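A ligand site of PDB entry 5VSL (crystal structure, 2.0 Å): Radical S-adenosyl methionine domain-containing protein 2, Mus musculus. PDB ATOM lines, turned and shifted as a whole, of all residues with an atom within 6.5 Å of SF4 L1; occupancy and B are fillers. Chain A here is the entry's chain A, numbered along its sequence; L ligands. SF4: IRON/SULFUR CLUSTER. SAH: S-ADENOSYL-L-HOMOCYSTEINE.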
ATOM      1  N   ARG A  38      21.206  23.844  12.894  1.00  0.00           N
ATOM      2  CA  ARG A  38      21.699  22.510  12.592  1.00  0.00           C
ATOM      3  C   ARG A  38      20.910  21.815  11.496  1.00  0.00           C
ATOM      4  O   ARG A  38      21.243  20.693  11.121  1.00  0.00           O
ATOM      5  CB  ARG A  38      21.719  21.638  13.852  1.00  0.00           C
ATOM      6  CG  ARG A  38      22.823  22.011  14.838  1.00  0.00           C
ATOM      7  CD  ARG A  38      22.757  21.140  16.095  1.00  0.00           C
ATOM      8  NE  ARG A  38      23.882  21.337  16.996  1.00  0.00           N
ATOM      9  CZ  ARG A  38      25.062  20.709  16.882  1.00  0.00           C
ATOM     10  NH1 ARG A  38      25.270  19.869  15.875  1.00  0.00           N
ATOM     11  NH2 ARG A  38      26.024  20.926  17.773  1.00  0.00           N
ATOM     12  N   GLN A  39      19.857  22.443  10.970  1.00  0.00           N
ATOM     13  CA  GLN A  39      19.097  21.858   9.876  1.00  0.00           C
ATOM     14  C   GLN A  39      19.866  21.968   8.569  1.00  0.00           C
ATOM     15  O   GLN A  39      20.565  22.959   8.304  1.00  0.00           O
ATOM     16  CB  GLN A  39      17.737  22.548   9.740  1.00  0.00           C
ATOM     17  CG  GLN A  39      17.048  22.866  11.065  1.00  0.00           C
ATOM     18  CD  GLN A  39      15.926  23.876  10.909  1.00  0.00           C
ATOM     19  OE1 GLN A  39      15.492  24.197   9.790  1.00  0.00           O
ATOM     20  NE2 GLN A  39      15.438  24.405  12.036  1.00  0.00           N
ATOM     21  N   CYS A  40      19.718  20.948   7.727  1.00  0.00           N
ATOM     22  CA  CYS A  40      20.375  20.959   6.424  1.00  0.00           C
ATOM     23  C   CYS A  40      19.574  20.100   5.446  1.00  0.00           C
ATOM     24  O   CYS A  40      18.848  19.199   5.841  1.00  0.00           O
ATOM     25  CB  CYS A  40      21.812  20.459   6.510  1.00  0.00           C
ATOM     26  SG  CYS A  40      22.661  20.669   4.949  1.00  0.00           S
ATOM     27  N   ASN A  41      19.717  20.409   4.150  1.00  0.00           N
ATOM     28  CA  ASN A  41      19.075  19.631   3.091  1.00  0.00           C
ATOM     29  C   ASN A  41      20.002  18.601   2.458  1.00  0.00           C
ATOM     30  O   ASN A  41      19.552  17.788   1.643  1.00  0.00           O
ATOM     31  CB  ASN A  41      18.533  20.563   1.976  1.00  0.00           C
ATOM     32  CG  ASN A  41      19.631  21.341   1.262  1.00  0.00           C
ATOM     33  OD1 ASN A  41      20.621  21.736   1.866  1.00  0.00           O
ATOM     34  ND2 ASN A  41      19.469  21.544  -0.055  1.00  0.00           N
ATOM     35  N   TYR A  42      21.291  18.604   2.794  1.00  0.00           N
ATOM     36  CA  TYR A  42      22.214  17.609   2.287  1.00  0.00           C
ATOM     37  C   TYR A  42      22.421  16.526   3.330  1.00  0.00           C
ATOM     38  O   TYR A  42      21.934  16.624   4.462  1.00  0.00           O
ATOM     39  CB  TYR A  42      23.562  18.220   1.906  1.00  0.00           C
ATOM     40  CG  TYR A  42      23.621  18.890   0.549  1.00  0.00           C
ATOM     41  CD1 TYR A  42      22.478  19.105  -0.207  1.00  0.00           C
ATOM     42  CD2 TYR A  42      24.843  19.313   0.020  1.00  0.00           C
ATOM     43  CE1 TYR A  42      22.533  19.717  -1.455  1.00  0.00           C
ATOM     44  CE2 TYR A  42      24.916  19.923  -1.206  1.00  0.00           C
ATOM     45  CZ  TYR A  42      23.756  20.129  -1.939  1.00  0.00           C
ATOM     46  OH  TYR A  42      23.857  20.726  -3.171  1.00  0.00           O
ATOM     47  N   LYS A  43      23.211  15.513   2.969  1.00  0.00           N
ATOM     48  CA  LYS A  43      23.435  14.352   3.826  1.00  0.00           C
ATOM     49  C   LYS A  43      24.888  13.910   3.782  1.00  0.00           C
ATOM     50  O   LYS A  43      25.184  12.711   3.728  1.00  0.00           O
ATOM     51  CB  LYS A  43      22.561  13.170   3.403  1.00  0.00           C
ATOM     52  CG  LYS A  43      21.072  13.428   3.372  1.00  0.00           C
ATOM     53  CD  LYS A  43      20.456  13.407   4.741  1.00  0.00           C
ATOM     54  CE  LYS A  43      18.934  13.311   4.621  1.00  0.00           C
ATOM     55  NZ  LYS A  43      18.230  13.785   5.840  1.00  0.00           N
ATOM     56  N   CYS A  44      25.825  14.860   3.804  1.00  0.00           N
ATOM     57  CA  CYS A  44      27.251  14.528   3.709  1.00  0.00           C
ATOM     58  C   CYS A  44      27.649  13.506   4.771  1.00  0.00           C
ATOM     59  O   CYS A  44      27.413  13.697   5.968  1.00  0.00           O
ATOM     60  CB  CYS A  44      28.085  15.797   3.858  1.00  0.00           C
ATOM     61  SG  CYS A  44      27.652  17.082   2.648  1.00  0.00           S
ATOM     62  N   GLY A  45      28.255  12.400   4.327  1.00  0.00           N
ATOM     63  CA  GLY A  45      28.540  11.305   5.230  1.00  0.00           C
ATOM     64  C   GLY A  45      29.478  11.663   6.372  1.00  0.00           C
ATOM     65  O   GLY A  45      29.464  11.005   7.426  1.00  0.00           O
ATOM     66  N   PHE A  46      30.310  12.686   6.174  1.00  0.00           N
ATOM     67  CA  PHE A  46      31.316  13.087   7.160  1.00  0.00           C
ATOM     68  C   PHE A  46      30.911  14.295   7.998  1.00  0.00           C
ATOM     69  O   PHE A  46      31.696  14.718   8.857  1.00  0.00           O
ATOM     70  CB  PHE A  46      32.660  13.372   6.465  1.00  0.00           C
ATOM     71  CG  PHE A  46      32.549  14.396   5.348  1.00  0.00           C
ATOM     72  CD1 PHE A  46      32.285  15.731   5.624  1.00  0.00           C
ATOM     73  CD2 PHE A  46      32.696  14.008   4.027  1.00  0.00           C
ATOM     74  CE1 PHE A  46      32.160  16.662   4.595  1.00  0.00           C
ATOM     75  CE2 PHE A  46      32.591  14.932   3.000  1.00  0.00           C
ATOM     76  CZ  PHE A  46      32.322  16.260   3.288  1.00  0.00           C
ATOM     77  N   CYS A  47      29.730  14.851   7.758  1.00  0.00           N
ATOM     78  CA  CYS A  47      29.299  16.094   8.398  1.00  0.00           C
ATOM     79  C   CYS A  47      29.631  16.122   9.884  1.00  0.00           C
ATOM     80  O   CYS A  47      29.230  15.240  10.636  1.00  0.00           O
ATOM     81  CB  CYS A  47      27.803  16.277   8.201  1.00  0.00           C
ATOM     82  SG  CYS A  47      27.204  17.724   9.060  1.00  0.00           S
ATOM     83  N   PHE A  48      30.405  17.123  10.313  1.00  0.00           N
ATOM     84  CA  PHE A  48      30.828  17.191  11.708  1.00  0.00           C
ATOM     85  C   PHE A  48      29.995  18.168  12.535  1.00  0.00           C
ATOM     86  O   PHE A  48      30.335  18.449  13.691  1.00  0.00           O
ATOM     87  CB  PHE A  48      32.323  17.525  11.803  1.00  0.00           C
ATOM     88  CG  PHE A  48      32.692  18.968  11.486  1.00  0.00           C
ATOM     89  CD1 PHE A  48      33.952  19.450  11.824  1.00  0.00           C
ATOM     90  CD2 PHE A  48      31.795  19.844  10.875  1.00  0.00           C
ATOM     91  CE1 PHE A  48      34.301  20.767  11.541  1.00  0.00           C
ATOM     92  CE2 PHE A  48      32.131  21.158  10.604  1.00  0.00           C
ATOM     93  CZ  PHE A  48      33.393  21.618  10.948  1.00  0.00           C
ATOM     94  N   HIS A  49      28.891  18.678  11.989  1.00  0.00           N
ATOM     95  CA  HIS A  49      27.978  19.555  12.737  1.00  0.00           C
ATOM     96  C   HIS A  49      26.543  19.169  12.368  1.00  0.00           C
ATOM     97  O   HIS A  49      25.908  19.840  11.551  1.00  0.00           O
ATOM     98  CB  HIS A  49      28.254  21.033  12.491  1.00  0.00           C
ATOM     99  CG  HIS A  49      27.714  21.907  13.583  1.00  0.00           C
ATOM    100  ND1 HIS A  49      28.329  22.030  14.812  1.00  0.00           N
ATOM    101  CD2 HIS A  49      26.578  22.637  13.650  1.00  0.00           C
ATOM    102  CE1 HIS A  49      27.605  22.815  15.581  1.00  0.00           C
ATOM    103  NE2 HIS A  49      26.539  23.208  14.902  1.00  0.00           N
ATOM    104  N   THR A  50      26.037  18.111  13.010  1.00  0.00           N
ATOM    105  CA  THR A  50      24.904  17.339  12.528  1.00  0.00           C
ATOM    106  C   THR A  50      23.566  17.880  13.036  1.00  0.00           C
ATOM    107  O   THR A  50      23.498  18.759  13.901  1.00  0.00           O
ATOM    108  CB  THR A  50      25.073  15.868  12.930  1.00  0.00           C
ATOM    109  OG1 THR A  50      25.161  15.767  14.351  1.00  0.00           O
ATOM    110  CG2 THR A  50      26.329  15.296  12.304  1.00  0.00           C
ATOM    111  N   GLY A  81      26.489  26.358   9.761  1.00  0.00           N
ATOM    112  CA  GLY A  81      25.487  25.464  10.312  1.00  0.00           C
ATOM    113  C   GLY A  81      25.908  24.000  10.284  1.00  0.00           C
ATOM    114  O   GLY A  81      27.060  23.694  10.629  1.00  0.00           O
ATOM    115  N   GLY A  82      25.039  23.090   9.847  1.00  0.00           N
ATOM    116  CA  GLY A  82      23.741  23.415   9.274  1.00  0.00           C
ATOM    117  C   GLY A  82      23.854  24.084   7.909  1.00  0.00           C
ATOM    118  O   GLY A  82      24.955  24.416   7.484  1.00  0.00           O
ATOM    119  N   GLU A  83      22.737  24.307   7.223  1.00  0.00           N
ATOM    120  CA  GLU A  83      22.772  25.073   5.984  1.00  0.00           C
ATOM    121  C   GLU A  83      22.185  26.455   6.239  1.00  0.00           C
ATOM    122  O   GLU A  83      20.964  26.575   6.472  1.00  0.00           O
ATOM    123  CB  GLU A  83      21.999  24.357   4.874  1.00  0.00           C
ATOM    124  CG  GLU A  83      21.838  25.196   3.609  1.00  0.00           C
ATOM    125  CD  GLU A  83      23.125  25.883   3.174  1.00  0.00           C
ATOM    126  OE1 GLU A  83      24.199  25.230   3.137  1.00  0.00           O
ATOM    127  OE2 GLU A  83      23.062  27.093   2.869  1.00  0.00           O
ATOM    128  N   SER A 113      28.244  28.012   2.853  1.00  0.00           N
ATOM    129  CA  SER A 113      26.994  27.426   2.389  1.00  0.00           C
ATOM    130  C   SER A 113      27.284  26.251   1.456  1.00  0.00           C
ATOM    131  O   SER A 113      28.300  26.255   0.757  1.00  0.00           O
ATOM    132  CB  SER A 113      26.138  28.483   1.646  1.00  0.00           C
ATOM    133  OG  SER A 113      24.938  27.930   1.132  1.00  0.00           O
ATOM    134  N   ASN A 114      26.364  25.258   1.425  1.00  0.00           N
ATOM    135  CA  ASN A 114      26.452  24.271   0.352  1.00  0.00           C
ATOM    136  C   ASN A 114      25.964  24.832  -0.991  1.00  0.00           C
ATOM    137  O   ASN A 114      26.116  24.155  -2.013  1.00  0.00           O
ATOM    138  CB  ASN A 114      25.716  22.954   0.717  1.00  0.00           C
ATOM    139  CG  ASN A 114      24.184  23.099   0.779  1.00  0.00           C
ATOM    140  OD1 ASN A 114      23.578  23.889   0.076  1.00  0.00           O
ATOM    141  ND2 ASN A 114      23.557  22.277   1.622  1.00  0.00           N
ATOM    142  N   SER A 136      30.891  25.255  -0.211  1.00  0.00           N
ATOM    143  CA  SER A 136      31.538  23.960  -0.010  1.00  0.00           C
ATOM    144  C   SER A 136      31.487  23.159  -1.305  1.00  0.00           C
ATOM    145  O   SER A 136      30.419  22.919  -1.861  1.00  0.00           O
ATOM    146  CB  SER A 136      30.857  23.177   1.111  1.00  0.00           C
ATOM    147  OG  SER A 136      31.047  23.889   2.321  1.00  0.00           O
ATOM    148  N   GLY A 149      27.512  12.205  -0.415  1.00  0.00           N
ATOM    149  CA  GLY A 149      26.293  12.776   0.098  1.00  0.00           C
ATOM    150  C   GLY A 149      26.088  14.248  -0.191  1.00  0.00           C
ATOM    151  O   GLY A 149      25.137  14.826   0.338  1.00  0.00           O
ATOM    152  N   ARG A 150      26.934  14.853  -1.020  1.00  0.00           N
ATOM    153  CA  ARG A 150      26.925  16.293  -1.254  1.00  0.00           C
ATOM    154  C   ARG A 150      25.988  16.569  -2.426  1.00  0.00           C
ATOM    155  O   ARG A 150      26.411  16.759  -3.577  1.00  0.00           O
ATOM    156  CB  ARG A 150      28.355  16.793  -1.508  1.00  0.00           C
ATOM    157  CG  ARG A 150      28.472  18.286  -1.731  1.00  0.00           C
ATOM    158  CD  ARG A 150      28.371  19.078  -0.449  1.00  0.00           C
ATOM    159  NE  ARG A 150      29.592  19.031   0.346  1.00  0.00           N
ATOM    160  CZ  ARG A 150      29.787  19.790   1.408  1.00  0.00           C
ATOM    161  NH1 ARG A 150      28.830  20.619   1.784  1.00  0.00           N
ATOM    162  NH2 ARG A 150      30.912  19.714   2.115  1.00  0.00           N
ATOM    163  N   VAL A 180      36.486  19.682   2.000  1.00  0.00           N
ATOM    164  CA  VAL A 180      36.853  18.706   3.018  1.00  0.00           C
ATOM    165  C   VAL A 180      37.614  17.585   2.333  1.00  0.00           C
ATOM    166  O   VAL A 180      37.066  16.899   1.470  1.00  0.00           O
ATOM    167  CB  VAL A 180      35.615  18.168   3.755  1.00  0.00           C
ATOM    168  CG1 VAL A 180      36.019  17.085   4.762  1.00  0.00           C
ATOM    169  CG2 VAL A 180      34.892  19.311   4.456  1.00  0.00           C
ATOM    170  N   ARG A 221      26.031  10.760  12.079  1.00  0.00           N
ATOM    171  CA  ARG A 221      26.950  10.374  11.018  1.00  0.00           C
ATOM    172  C   ARG A 221      28.058   9.550  11.641  1.00  0.00           C
ATOM    173  O   ARG A 221      28.329   9.661  12.843  1.00  0.00           O
ATOM    174  CB  ARG A 221      27.542  11.607  10.288  1.00  0.00           C
ATOM    175  CG  ARG A 221      26.512  12.556   9.664  1.00  0.00           C
ATOM    176  CD  ARG A 221      25.873  11.978   8.404  1.00  0.00           C
ATOM    177  NE  ARG A 221      24.468  12.340   8.264  1.00  0.00           N
ATOM    178  CZ  ARG A 221      24.022  13.474   7.719  1.00  0.00           C
ATOM    179  NH1 ARG A 221      24.872  14.400   7.269  1.00  0.00           N
ATOM    180  NH2 ARG A 221      22.716  13.691   7.643  1.00  0.00           N
HETATM  181 FE1  SF4 L   1      24.873  19.948   5.461  1.00  0.00          FE
HETATM  182 FE2  SF4 L   1      26.962  18.661   4.330  1.00  0.00          FE
HETATM  183 FE3  SF4 L   1      26.846  18.943   6.926  1.00  0.00          FE
HETATM  184 FE4  SF4 L   1      27.155  21.259   5.245  1.00  0.00          FE
HETATM  185  S1  SF4 L   1      28.573  19.318   5.688  1.00  0.00           S
HETATM  186  S2  SF4 L   1      25.770  20.866   7.266  1.00  0.00           S
HETATM  187  S3  SF4 L   1      25.957  20.562   3.484  1.00  0.00           S
HETATM  188  S4  SF4 L   1      25.329  17.694   5.735  1.00  0.00           S
HETATM  189  N   SAH L   2      26.247  23.632   5.319  1.00  0.00           N
HETATM  190  CA  SAH L   2      27.305  24.587   4.918  1.00  0.00           C
HETATM  191  CB  SAH L   2      28.095  25.090   6.130  1.00  0.00           C
HETATM  192  CG  SAH L   2      28.022  24.154   7.342  1.00  0.00           C
HETATM  193  SD  SAH L   2      29.363  23.020   7.362  1.00  0.00           S
HETATM  194  C   SAH L   2      28.238  23.966   3.912  1.00  0.00           C
HETATM  195  O   SAH L   2      28.302  22.754   3.710  1.00  0.00           O
HETATM  196  OXT SAH L   2      28.974  24.681   3.247  1.00  0.00           O
HETATM  197  C5' SAH L   2      30.673  24.197   7.633  1.00  0.00           C
HETATM  198  C4' SAH L   2      31.981  23.776   6.946  1.00  0.00           C
HETATM  199  O4' SAH L   2      32.532  22.668   7.663  1.00  0.00           O
HETATM  200  C3' SAH L   2      31.780  23.328   5.497  1.00  0.00           C
HETATM  201  O3' SAH L   2      32.833  23.741   4.592  1.00  0.00           O
HETATM  202  C2' SAH L   2      31.843  21.831   5.644  1.00  0.00           C
HETATM  203  O2' SAH L   2      32.093  21.168   4.402  1.00  0.00           O
HETATM  204  C1' SAH L   2      32.918  21.717   6.713  1.00  0.00           C
HETATM  205  N9  SAH L   2      32.900  20.355   7.287  1.00  0.00           N
HETATM  206  C8  SAH L   2      31.821  19.576   7.442  1.00  0.00           C
HETATM  207  N7  SAH L   2      32.170  18.377   7.971  1.00  0.00           N
HETATM  208  C5  SAH L   2      33.497  18.403   8.157  1.00  0.00           C
HETATM  209  C6  SAH L   2      34.499  17.465   8.694  1.00  0.00           C
HETATM  210  N6  SAH L   2      34.119  16.232   9.118  1.00  0.00           N
HETATM  211  N1  SAH L   2      35.793  17.876   8.731  1.00  0.00           N
HETATM  212  C2  SAH L   2      36.161  19.100   8.298  1.00  0.00           C
HETATM  213  N3  SAH L   2      35.301  20.006   7.815  1.00  0.00           N
HETATM  214  C4  SAH L   2      33.982  19.714   7.724  1.00  0.00           C
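N of Gly 82 sits close to S2 of SF4 L1, 3.5 Å away. FE2 of SF4 L1 is bound by SG of Cys 44 (2.4 Å). The side-chain sulfur of Cys 40 is bound to an iron atom (FE1) of SF4 L1 (2.4 Å). N of Phe 48 lies within hydrogen-bond range of N7 of SAH L2 (3.2 Å). The backbone carbonyl oxygen (O) of Gly 82 lies close to a nitrogen (N) of SAH L2 (2.6 Å). The side-chain sulfur (SG) of Cys 47 binds an iron atom (FE3) of SF4 L1, at 2.5 Å. The backbone NH (N) of Cys 44 sits close to a sulfur (S4) of SF4 L1, 3.5 Å away. A nitrogen (N6) of SAH L2 is in hydrogen-bond range of the backbone carbonyl oxygen of Phe 46 (2.9 Å). The side-chain amide nitrogen (ND2) of Asn 114 lies close to a sulfur (S3) of SF4 L1 (3.5 Å). N of Asn 114 is in hydrogen-bond range of OXT of SAH L2, at 3.2 Å. The backbone NH (N) of Ser 113 sits close to an oxygen (OXT) of SAH L2 (3.4 Å). The side-chain hydroxyl of Ser 136 is in hydrogen-bond range of an oxygen (OXT) of SAH L2, at 2.4 Å. O of Ser 113 sits close to OXT of SAH L2, 3.0 Å away. OE1 of Glu 83 lies close to N of SAH L2, 3.4 Å away. The guanidinium group (NH1) of Arg 150 lies close to a sulfur (S3) of SF4 L1 (3.3 Å). NH1 of Arg 221 lies close to S4 of SF4 L1 (3.7 Å). NH2 of Arg 150 is in hydrogen-bond range of O2' of SAH L2, 3.0 Å away.
O of SAH L2 binds FE4 of SF4 L1, 2.4 Å away.
The backbone carbonyl oxygen (O) of Cys 44 lies within hydrogen-bond range of the guanidinium group (NH1) of Arg 221. The side-chain sulfur of Cys 40 lies close to the backbone NH of Tyr 42. The side-chain carboxylate (OE1) of Glu 83 sits at hydrogen-bond distance from the backbone NH (N) of Asn 114, at 2.8 Å. The side-chain amide oxygen (OD1) of Asn 41 is in hydrogen-bond range of the side-chain amide nitrogen (ND2) of Asn 114 (3.0 Å). The side-chain sulfur (SG) of Cys 47 sits close to the backbone NH (N) of His 49 (3.5 Å). The guanidinium group (NE) of Arg 150 lies close to the side-chain sulfur (SG) of Cys 44 (3.6 Å).
The backbone carbonyl oxygen (O) of Tyr 42 lies close to a sulfur (S4) of SF4 L1, at 3.8 Å. Hydrophobic or aromatic side chains within 4 Å of SF4 L1: Tyr 42. Within 4 Å of SF4 L1: Cys 40, Tyr 42, Cys 44, Cys 47, Gly 82, Asn 114, Arg 150 and Arg 221.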
